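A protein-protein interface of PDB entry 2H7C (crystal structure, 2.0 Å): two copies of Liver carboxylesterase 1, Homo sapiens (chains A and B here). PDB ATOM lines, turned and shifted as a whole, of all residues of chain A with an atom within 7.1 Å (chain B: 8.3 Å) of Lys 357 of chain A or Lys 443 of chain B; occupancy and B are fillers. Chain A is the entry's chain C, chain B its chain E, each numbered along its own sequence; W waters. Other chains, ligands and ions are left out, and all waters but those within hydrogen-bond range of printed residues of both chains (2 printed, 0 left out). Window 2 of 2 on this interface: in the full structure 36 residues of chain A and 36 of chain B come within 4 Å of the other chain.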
ATOM      1  N   GLN A 353      25.551  -0.326  -8.041  1.00  0.00           N
ATOM      2  CA  GLN A 353      24.362  -0.623  -8.833  1.00  0.00           C
ATOM      3  C   GLN A 353      23.407  -1.411  -7.931  1.00  0.00           C
ATOM      4  O   GLN A 353      23.772  -1.793  -6.813  1.00  0.00           O
ATOM      5  CB  GLN A 353      24.735  -1.457 -10.052  1.00  0.00           C
ATOM      6  CG  GLN A 353      25.755  -2.530  -9.775  1.00  0.00           C
ATOM      7  CD  GLN A 353      26.960  -2.420 -10.696  1.00  0.00           C
ATOM      8  OE1 GLN A 353      28.004  -3.051 -10.462  1.00  0.00           O
ATOM      9  NE2 GLN A 353      26.829  -1.590 -11.734  1.00  0.00           N
ATOM     10  N   LEU A 354      22.189  -1.663  -8.401  1.00  0.00           N
ATOM     11  CA  LEU A 354      21.231  -2.382  -7.574  1.00  0.00           C
ATOM     12  C   LEU A 354      19.962  -2.802  -8.301  1.00  0.00           C
ATOM     13  O   LEU A 354      19.223  -1.968  -8.816  1.00  0.00           O
ATOM     14  CB  LEU A 354      20.858  -1.515  -6.369  1.00  0.00           C
ATOM     15  CG  LEU A 354      20.093  -2.175  -5.223  1.00  0.00           C
ATOM     16  CD1 LEU A 354      21.014  -3.122  -4.465  1.00  0.00           C
ATOM     17  CD2 LEU A 354      19.568  -1.102  -4.290  1.00  0.00           C
ATOM     18  N   ASP A 355      19.712  -4.104  -8.325  1.00  0.00           N
ATOM     19  CA  ASP A 355      18.509  -4.632  -8.952  1.00  0.00           C
ATOM     20  C   ASP A 355      17.431  -4.622  -7.871  1.00  0.00           C
ATOM     21  O   ASP A 355      17.748  -4.636  -6.680  1.00  0.00           O
ATOM     22  CB  ASP A 355      18.752  -6.057  -9.452  1.00  0.00           C
ATOM     23  CG  ASP A 355      19.440  -6.925  -8.420  1.00  0.00           C
ATOM     24  OD1 ASP A 355      20.644  -6.701  -8.162  1.00  0.00           O
ATOM     25  OD2 ASP A 355      18.777  -7.824  -7.863  1.00  0.00           O
ATOM     26  N   GLN A 356      16.165  -4.594  -8.275  1.00  0.00           N
ATOM     27  CA  GLN A 356      15.078  -4.558  -7.307  1.00  0.00           C
ATOM     28  C   GLN A 356      15.057  -5.723  -6.335  1.00  0.00           C
ATOM     29  O   GLN A 356      14.594  -5.580  -5.205  1.00  0.00           O
ATOM     30  CB  GLN A 356      13.728  -4.453  -8.016  1.00  0.00           C
ATOM     31  CG  GLN A 356      13.495  -3.092  -8.646  1.00  0.00           C
ATOM     32  CD  GLN A 356      12.029  -2.784  -8.863  1.00  0.00           C
ATOM     33  OE1 GLN A 356      11.679  -1.706  -9.336  1.00  0.00           O
ATOM     34  NE2 GLN A 356      11.164  -3.729  -8.515  1.00  0.00           N
ATOM     35  N   LYS A 357      15.561  -6.874  -6.764  1.00  0.00           N
ATOM     36  CA  LYS A 357      15.584  -8.042  -5.893  1.00  0.00           C
ATOM     37  C   LYS A 357      16.545  -7.813  -4.727  1.00  0.00           C
ATOM     38  O   LYS A 357      16.208  -8.077  -3.573  1.00  0.00           O
ATOM     39  CB  LYS A 357      16.005  -9.284  -6.680  1.00  0.00           C
ATOM     40  CG  LYS A 357      15.985 -10.563  -5.860  1.00  0.00           C
ATOM     41  CD  LYS A 357      16.196 -11.787  -6.737  1.00  0.00           C
ATOM     42  CE  LYS A 357      15.948 -13.069  -5.957  1.00  0.00           C
ATOM     43  NZ  LYS A 357      16.077 -14.276  -6.817  1.00  0.00           N
ATOM     44  N   THR A 358      17.740  -7.323  -5.038  1.00  0.00           N
ATOM     45  CA  THR A 358      18.744  -7.043  -4.017  1.00  0.00           C
ATOM     46  C   THR A 358      18.220  -5.928  -3.117  1.00  0.00           C
ATOM     47  O   THR A 358      18.417  -5.949  -1.901  1.00  0.00           O
ATOM     48  CB  THR A 358      20.076  -6.575  -4.653  1.00  0.00           C
ATOM     49  OG1 THR A 358      20.490  -7.520  -5.648  1.00  0.00           O
ATOM     50  CG2 THR A 358      21.166  -6.457  -3.592  1.00  0.00           C
ATOM     51  N   ALA A 359      17.547  -4.962  -3.735  1.00  0.00           N
ATOM     52  CA  ALA A 359      16.976  -3.820  -3.029  1.00  0.00           C
ATOM     53  C   ALA A 359      16.012  -4.259  -1.932  1.00  0.00           C
ATOM     54  O   ALA A 359      16.083  -3.777  -0.797  1.00  0.00           O
ATOM     55  CB  ALA A 359      16.260  -2.908  -4.017  1.00  0.00           C
ATOM     56  N   MET A 360      15.107  -5.169  -2.273  1.00  0.00           N
ATOM     57  CA  MET A 360      14.137  -5.665  -1.308  1.00  0.00           C
ATOM     58  C   MET A 360      14.816  -6.356  -0.132  1.00  0.00           C
ATOM     59  O   MET A 360      14.351  -6.262   0.999  1.00  0.00           O
ATOM     60  CB  MET A 360      13.168  -6.637  -1.973  1.00  0.00           C
ATOM     61  CG  MET A 360      12.276  -6.001  -3.023  1.00  0.00           C
ATOM     62  SD  MET A 360      11.019  -7.160  -3.595  1.00  0.00           S
ATOM     63  CE  MET A 360      11.865  -7.913  -4.992  1.00  0.00           C
ATOM     64  N   SER A 361      15.913  -7.055  -0.405  1.00  0.00           N
ATOM     65  CA  SER A 361      16.643  -7.757   0.646  1.00  0.00           C
ATOM     66  C   SER A 361      17.295  -6.772   1.601  1.00  0.00           C
ATOM     67  O   SER A 361      17.262  -6.957   2.814  1.00  0.00           O
ATOM     68  CB  SER A 361      17.714  -8.669   0.044  1.00  0.00           C
ATOM     69  OG  SER A 361      17.121  -9.733  -0.679  1.00  0.00           O
ATOM     70  N   LEU A 362      17.896  -5.727   1.046  1.00  0.00           N
ATOM     71  CA  LEU A 362      18.547  -4.712   1.859  1.00  0.00           C
ATOM     72  C   LEU A 362      17.520  -3.943   2.689  1.00  0.00           C
ATOM     73  O   LEU A 362      17.781  -3.601   3.841  1.00  0.00           O
ATOM     74  CB  LEU A 362      19.331  -3.739   0.971  1.00  0.00           C
ATOM     75  CG  LEU A 362      20.609  -4.256   0.304  1.00  0.00           C
ATOM     76  CD1 LEU A 362      21.201  -3.153  -0.574  1.00  0.00           C
ATOM     77  CD2 LEU A 362      21.617  -4.686   1.366  1.00  0.00           C
ATOM     78  N   THR A 381       9.423  -0.801  -2.498  1.00  0.00           N
ATOM     79  CA  THR A 381      10.522  -0.884  -3.454  1.00  0.00           C
ATOM     80  C   THR A 381      10.049  -0.546  -4.872  1.00  0.00           C
ATOM     81  O   THR A 381      10.684   0.241  -5.579  1.00  0.00           O
ATOM     82  CB  THR A 381      11.145  -2.288  -3.443  1.00  0.00           C
ATOM     83  OG1 THR A 381      11.433  -2.666  -2.090  1.00  0.00           O
ATOM     84  CG2 THR A 381      12.440  -2.301  -4.240  1.00  0.00           C
ATOM     85  N   LEU A 385      11.823   2.319  -7.081  1.00  0.00           N
ATOM     86  CA  LEU A 385      12.706   1.838  -8.139  1.00  0.00           C
ATOM     87  C   LEU A 385      12.034   1.373  -9.427  1.00  0.00           C
ATOM     88  O   LEU A 385      12.677   1.321 -10.476  1.00  0.00           O
ATOM     89  CB  LEU A 385      13.579   0.699  -7.605  1.00  0.00           C
ATOM     90  CG  LEU A 385      14.097   0.784  -6.167  1.00  0.00           C
ATOM     91  CD1 LEU A 385      15.154  -0.288  -5.974  1.00  0.00           C
ATOM     92  CD2 LEU A 385      14.683   2.151  -5.877  1.00  0.00           C
ATOM     93  N   LYS A 394      18.690   3.016  -9.725  1.00  0.00           N
ATOM     94  CA  LYS A 394      17.801   2.383  -8.762  1.00  0.00           C
ATOM     95  C   LYS A 394      18.390   2.452  -7.362  1.00  0.00           C
ATOM     96  O   LYS A 394      17.663   2.630  -6.386  1.00  0.00           O
ATOM     97  CB  LYS A 394      17.558   0.917  -9.133  1.00  0.00           C
ATOM     98  CG  LYS A 394      16.672   0.713 -10.344  1.00  0.00           C
ATOM     99  CD  LYS A 394      16.285  -0.751 -10.493  1.00  0.00           C
ATOM    100  CE  LYS A 394      15.230  -0.932 -11.571  1.00  0.00           C
ATOM    101  NZ  LYS A 394      14.741  -2.335 -11.641  1.00  0.00           N
ATOM    102  N   GLN B 335      36.349 -11.206 -10.047  1.00  0.00           N
ATOM    103  CA  GLN B 335      36.213  -9.975  -9.265  1.00  0.00           C
ATOM    104  C   GLN B 335      36.505 -10.228  -7.782  1.00  0.00           C
ATOM    105  O   GLN B 335      35.590 -10.212  -6.956  1.00  0.00           O
ATOM    106  CB  GLN B 335      34.796  -9.407  -9.400  1.00  0.00           C
ATOM    107  CG  GLN B 335      34.257  -9.328 -10.826  1.00  0.00           C
ATOM    108  CD  GLN B 335      32.828  -8.793 -10.886  1.00  0.00           C
ATOM    109  OE1 GLN B 335      32.054  -9.151 -11.778  1.00  0.00           O
ATOM    110  NE2 GLN B 335      32.480  -7.925  -9.943  1.00  0.00           N
ATOM    111  N   TRP B 339      32.605  -7.655  -4.029  1.00  0.00           N
ATOM    112  CA  TRP B 339      31.567  -7.403  -3.040  1.00  0.00           C
ATOM    113  C   TRP B 339      31.877  -7.907  -1.632  1.00  0.00           C
ATOM    114  O   TRP B 339      31.876  -7.131  -0.686  1.00  0.00           O
ATOM    115  CB  TRP B 339      30.246  -8.031  -3.497  1.00  0.00           C
ATOM    116  CG  TRP B 339      29.094  -7.734  -2.578  1.00  0.00           C
ATOM    117  CD1 TRP B 339      28.395  -6.565  -2.491  1.00  0.00           C
ATOM    118  CD2 TRP B 339      28.522  -8.616  -1.600  1.00  0.00           C
ATOM    119  NE1 TRP B 339      27.422  -6.662  -1.524  1.00  0.00           N
ATOM    120  CE2 TRP B 339      27.478  -7.910  -0.960  1.00  0.00           C
ATOM    121  CE3 TRP B 339      28.792  -9.935  -1.203  1.00  0.00           C
ATOM    122  CZ2 TRP B 339      26.701  -8.479   0.058  1.00  0.00           C
ATOM    123  CZ3 TRP B 339      28.017 -10.502  -0.189  1.00  0.00           C
ATOM    124  CH2 TRP B 339      26.984  -9.770   0.429  1.00  0.00           C
ATOM    125  N   ARG B 433      28.773 -16.838 -11.108  1.00  0.00           N
ATOM    126  CA  ARG B 433      28.022 -16.331  -9.965  1.00  0.00           C
ATOM    127  C   ARG B 433      27.161 -17.452  -9.399  1.00  0.00           C
ATOM    128  O   ARG B 433      26.157 -17.842  -9.993  1.00  0.00           O
ATOM    129  CB  ARG B 433      27.132 -15.151 -10.366  1.00  0.00           C
ATOM    130  CG  ARG B 433      26.451 -14.477  -9.173  1.00  0.00           C
ATOM    131  CD  ARG B 433      25.644 -13.260  -9.590  1.00  0.00           C
ATOM    132  NE  ARG B 433      25.115 -12.531  -8.436  1.00  0.00           N
ATOM    133  CZ  ARG B 433      24.199 -13.009  -7.601  1.00  0.00           C
ATOM    134  NH1 ARG B 433      23.697 -14.223  -7.784  1.00  0.00           N
ATOM    135  NH2 ARG B 433      23.782 -12.272  -6.579  1.00  0.00           N
ATOM    136  N   PRO B 434      27.551 -17.987  -8.233  1.00  0.00           N
ATOM    137  CA  PRO B 434      26.815 -19.073  -7.580  1.00  0.00           C
ATOM    138  C   PRO B 434      25.388 -18.663  -7.246  1.00  0.00           C
ATOM    139  O   PRO B 434      25.131 -17.509  -6.903  1.00  0.00           O
ATOM    140  CB  PRO B 434      27.634 -19.336  -6.315  1.00  0.00           C
ATOM    141  CG  PRO B 434      29.024 -18.906  -6.707  1.00  0.00           C
ATOM    142  CD  PRO B 434      28.750 -17.630  -7.456  1.00  0.00           C
ATOM    143  N   SER B 435      24.458 -19.601  -7.354  1.00  0.00           N
ATOM    144  CA  SER B 435      23.080 -19.296  -7.020  1.00  0.00           C
ATOM    145  C   SER B 435      23.016 -19.201  -5.495  1.00  0.00           C
ATOM    146  O   SER B 435      22.070 -18.661  -4.934  1.00  0.00           O
ATOM    147  CB  SER B 435      22.152 -20.404  -7.520  1.00  0.00           C
ATOM    148  OG  SER B 435      22.433 -21.633  -6.873  1.00  0.00           O
ATOM    149  N   SER B 437      24.830 -17.397  -3.704  1.00  0.00           N
ATOM    150  CA  SER B 437      25.311 -16.083  -3.290  1.00  0.00           C
ATOM    151  C   SER B 437      24.314 -15.449  -2.323  1.00  0.00           C
ATOM    152  O   SER B 437      23.146 -15.833  -2.280  1.00  0.00           O
ATOM    153  CB  SER B 437      25.489 -15.167  -4.509  1.00  0.00           C
ATOM    154  OG  SER B 437      26.500 -15.646  -5.384  1.00  0.00           O
ATOM    155  N   SER B 438      24.784 -14.481  -1.545  1.00  0.00           N
ATOM    156  CA  SER B 438      23.943 -13.778  -0.588  1.00  0.00           C
ATOM    157  C   SER B 438      22.924 -12.921  -1.333  1.00  0.00           C
ATOM    158  O   SER B 438      23.225 -12.364  -2.388  1.00  0.00           O
ATOM    159  CB  SER B 438      24.814 -12.893   0.308  1.00  0.00           C
ATOM    160  OG  SER B 438      24.036 -11.921   0.983  1.00  0.00           O
ATOM    161  N   ASP B 439      21.716 -12.814  -0.786  1.00  0.00           N
ATOM    162  CA  ASP B 439      20.673 -12.013  -1.418  1.00  0.00           C
ATOM    163  C   ASP B 439      21.038 -10.531  -1.462  1.00  0.00           C
ATOM    164  O   ASP B 439      20.469  -9.772  -2.242  1.00  0.00           O
ATOM    165  CB  ASP B 439      19.344 -12.187  -0.680  1.00  0.00           C
ATOM    166  CG  ASP B 439      18.757 -13.570  -0.857  1.00  0.00           C
ATOM    167  OD1 ASP B 439      18.474 -13.944  -2.014  1.00  0.00           O
ATOM    168  OD2 ASP B 439      18.577 -14.281   0.154  1.00  0.00           O
ATOM    169  N   MET B 440      21.991 -10.125  -0.631  1.00  0.00           N
ATOM    170  CA  MET B 440      22.419  -8.728  -0.580  1.00  0.00           C
ATOM    171  C   MET B 440      23.454  -8.383  -1.648  1.00  0.00           C
ATOM    172  O   MET B 440      23.780  -7.218  -1.855  1.00  0.00           O
ATOM    173  CB  MET B 440      22.996  -8.413   0.799  1.00  0.00           C
ATOM    174  CG  MET B 440      22.000  -8.566   1.939  1.00  0.00           C
ATOM    175  SD  MET B 440      22.797  -8.311   3.529  1.00  0.00           S
ATOM    176  CE  MET B 440      23.443  -9.950   3.845  1.00  0.00           C
ATOM    177  N   LYS B 441      23.970  -9.404  -2.317  1.00  0.00           N
ATOM    178  CA  LYS B 441      24.976  -9.229  -3.359  1.00  0.00           C
ATOM    179  C   LYS B 441      24.309  -8.946  -4.713  1.00  0.00           C
ATOM    180  O   LYS B 441      23.498  -9.738  -5.189  1.00  0.00           O
ATOM    181  CB  LYS B 441      25.815 -10.502  -3.426  1.00  0.00           C
ATOM    182  CG  LYS B 441      26.863 -10.575  -4.504  1.00  0.00           C
ATOM    183  CD  LYS B 441      27.431 -11.986  -4.501  1.00  0.00           C
ATOM    184  CE  LYS B 441      28.464 -12.210  -5.580  1.00  0.00           C
ATOM    185  NZ  LYS B 441      28.907 -13.634  -5.557  1.00  0.00           N
ATOM    186  N   PRO B 442      24.634  -7.802  -5.339  1.00  0.00           N
ATOM    187  CA  PRO B 442      24.053  -7.431  -6.640  1.00  0.00           C
ATOM    188  C   PRO B 442      24.241  -8.525  -7.691  1.00  0.00           C
ATOM    189  O   PRO B 442      25.281  -9.177  -7.740  1.00  0.00           O
ATOM    190  CB  PRO B 442      24.808  -6.154  -7.002  1.00  0.00           C
ATOM    191  CG  PRO B 442      25.075  -5.542  -5.662  1.00  0.00           C
ATOM    192  CD  PRO B 442      25.532  -6.740  -4.851  1.00  0.00           C
ATOM    193  N   LYS B 443      23.230  -8.719  -8.532  1.00  0.00           N
ATOM    194  CA  LYS B 443      23.287  -9.738  -9.574  1.00  0.00           C
ATOM    195  C   LYS B 443      24.462  -9.545 -10.525  1.00  0.00           C
ATOM    196  O   LYS B 443      24.957 -10.508 -11.106  1.00  0.00           O
ATOM    197  CB  LYS B 443      21.980  -9.745 -10.377  1.00  0.00           C
ATOM    198  CG  LYS B 443      20.757 -10.148  -9.563  1.00  0.00           C
ATOM    199  CD  LYS B 443      19.478 -10.095 -10.389  1.00  0.00           C
ATOM    200  CE  LYS B 443      18.270 -10.515  -9.556  1.00  0.00           C
ATOM    201  NZ  LYS B 443      16.992 -10.460 -10.323  1.00  0.00           N
ATOM    202  N   THR B 444      24.919  -8.306 -10.669  1.00  0.00           N
ATOM    203  CA  THR B 444      26.019  -8.004 -11.578  1.00  0.00           C
ATOM    204  C   THR B 444      27.418  -8.411 -11.112  1.00  0.00           C
ATOM    205  O   THR B 444      28.390  -8.254 -11.849  1.00  0.00           O
ATOM    206  CB  THR B 444      26.029  -6.507 -11.935  1.00  0.00           C
ATOM    207  OG1 THR B 444      26.006  -5.725 -10.733  1.00  0.00           O
ATOM    208  CG2 THR B 444      24.808  -6.161 -12.785  1.00  0.00           C
ATOM    209  N   VAL B 445      27.531  -8.930  -9.895  1.00  0.00           N
ATOM    210  CA  VAL B 445      28.830  -9.355  -9.393  1.00  0.00           C
ATOM    211  C   VAL B 445      29.050 -10.806  -9.796  1.00  0.00           C
ATOM    212  O   VAL B 445      28.262 -11.683  -9.445  1.00  0.00           O
ATOM    213  CB  VAL B 445      28.909  -9.230  -7.859  1.00  0.00           C
ATOM    214  CG1 VAL B 445      30.288  -9.648  -7.370  1.00  0.00           C
ATOM    215  CG2 VAL B 445      28.614  -7.800  -7.445  1.00  0.00           C
ATOM    216  N   ILE B 446      30.123 -11.053 -10.538  1.00  0.00           N
ATOM    217  CA  ILE B 446      30.433 -12.399 -11.006  1.00  0.00           C
ATOM    218  C   ILE B 446      31.878 -12.765 -10.689  1.00  0.00           C
ATOM    219  O   ILE B 446      32.798 -11.997 -10.956  1.00  0.00           O
ATOM    220  CB  ILE B 446      30.189 -12.511 -12.525  1.00  0.00           C
ATOM    221  CG1 ILE B 446      28.758 -12.060 -12.846  1.00  0.00           C
ATOM    222  CG2 ILE B 446      30.406 -13.949 -12.988  1.00  0.00           C
ATOM    223  CD1 ILE B 446      28.437 -12.010 -14.333  1.00  0.00           C
ATOM    224  N   GLY B 447      32.073 -13.943 -10.117  1.00  0.00           N
ATOM    225  CA  GLY B 447      33.415 -14.359  -9.759  1.00  0.00           C
ATOM    226  C   GLY B 447      33.944 -13.556  -8.579  1.00  0.00           C
ATOM    227  O   GLY B 447      35.099 -13.137  -8.561  1.00  0.00           O
HETATM  228  O   HOH W   1      15.467  -7.588  -9.952  1.00  0.00           O
HETATM  229  O   HOH W   2      20.545 -10.119  -5.397  1.00  0.00           O
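No position is printed for both chains.
Of the 10 pairs that touch across the chains among the printed residues, none has its exchanged pair printed and touching as well.
Water W2 lies within hydrogen-bond range of OG1 of Thr 358 of chain A, O of Lys 441 of chain B and O of Asp 439 of chain B.
Water W1 bridges N of Lys 357 of chain A and NZ of Lys 443 of chain B.
Asp 355 of chain A touches Pro 442 of chain B (OD1 to CA, 3.8 Å).
Lys 443 of chain B touches Lys 357 of chain A.
O of Asp 439 of chain B touches CG2 of Thr 358 of chain A, at 3.6 Å.
CG2 of Thr 358 of chain A touches O of Met 440 of chain B (3.2 Å).
Lys 441 of chain B touches Thr 358 of chain A (O to OG1, 3.8 Å).
CA of Pro 442 of chain B touches OG1 of Thr 358 of chain A, at 3.7 Å.
Ser 361 of chain A touches Asp 439 of chain B (OG to CB, 3.3 Å).
Leu 362 of chain A touches Met 440 of chain B.
NE of Arg 433 of chain B sits at hydrogen-bond distance from O of Pro 442 of chain B, 3.4 Å away.
The side-chain hydroxyl (OG) of Ser 438 of chain B sits close to the backbone NH (N) of Met 440 of chain B.
The side-chain amino group of Lys 441 of chain B lies within hydrogen-bond range of the side-chain hydroxyl of Ser 437 of chain B (3.1 Å).
The side-chain hydroxyl of Ser 361 of chain A is in hydrogen-bond range of the backbone carbonyl oxygen of Lys 357 of chain A (3.5 Å).
The guanidinium group (NE) of Arg 433 of chain B lies close to the backbone carbonyl oxygen (O) of Lys 443 of chain B.
OD1 of Asp 355 of chain A lies within hydrogen-bond range of OG1 of Thr 358 of chain A.
OG1 of Thr 444 of chain B sits close to OE1 of Gln 353 of chain A, at 3.3 Å.
OD1 of Asp 355 of chain A is in hydrogen-bond range of N of Lys 443 of chain B (3.3 Å).
Of the 13 printed residues of chain A, 6 touch a printed residue of chain B.
Of the 16 printed residues of chain B, 6 touch a printed residue of chain A.
Among the printed residues, 10 pairs touch across the chains.
Lys 357 of chain A touches one residue of chain B.
Of the printed residues of chain A, Lys 443 of chain B touches Asp 355 and Lys 357.
Printed residues of chain B within 4 Å of Ser 361 of chain A: Asp 439.
Of the printed residues of chain B, Leu 362 of chain A touches Met 440 (3.9 Å).
Printed residues of chain B within 4 Å of Gln 353 of chain A: Thr 444 (3.3 Å).
Met 360 of chain A touches none of the printed residues of chain B.
Thr 381 of chain A touches none of the printed residues of chain B.
The nearest residue of chain B that does not touch Lys 357 of chain A is Asp 439 of chain B (4.8 Å).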
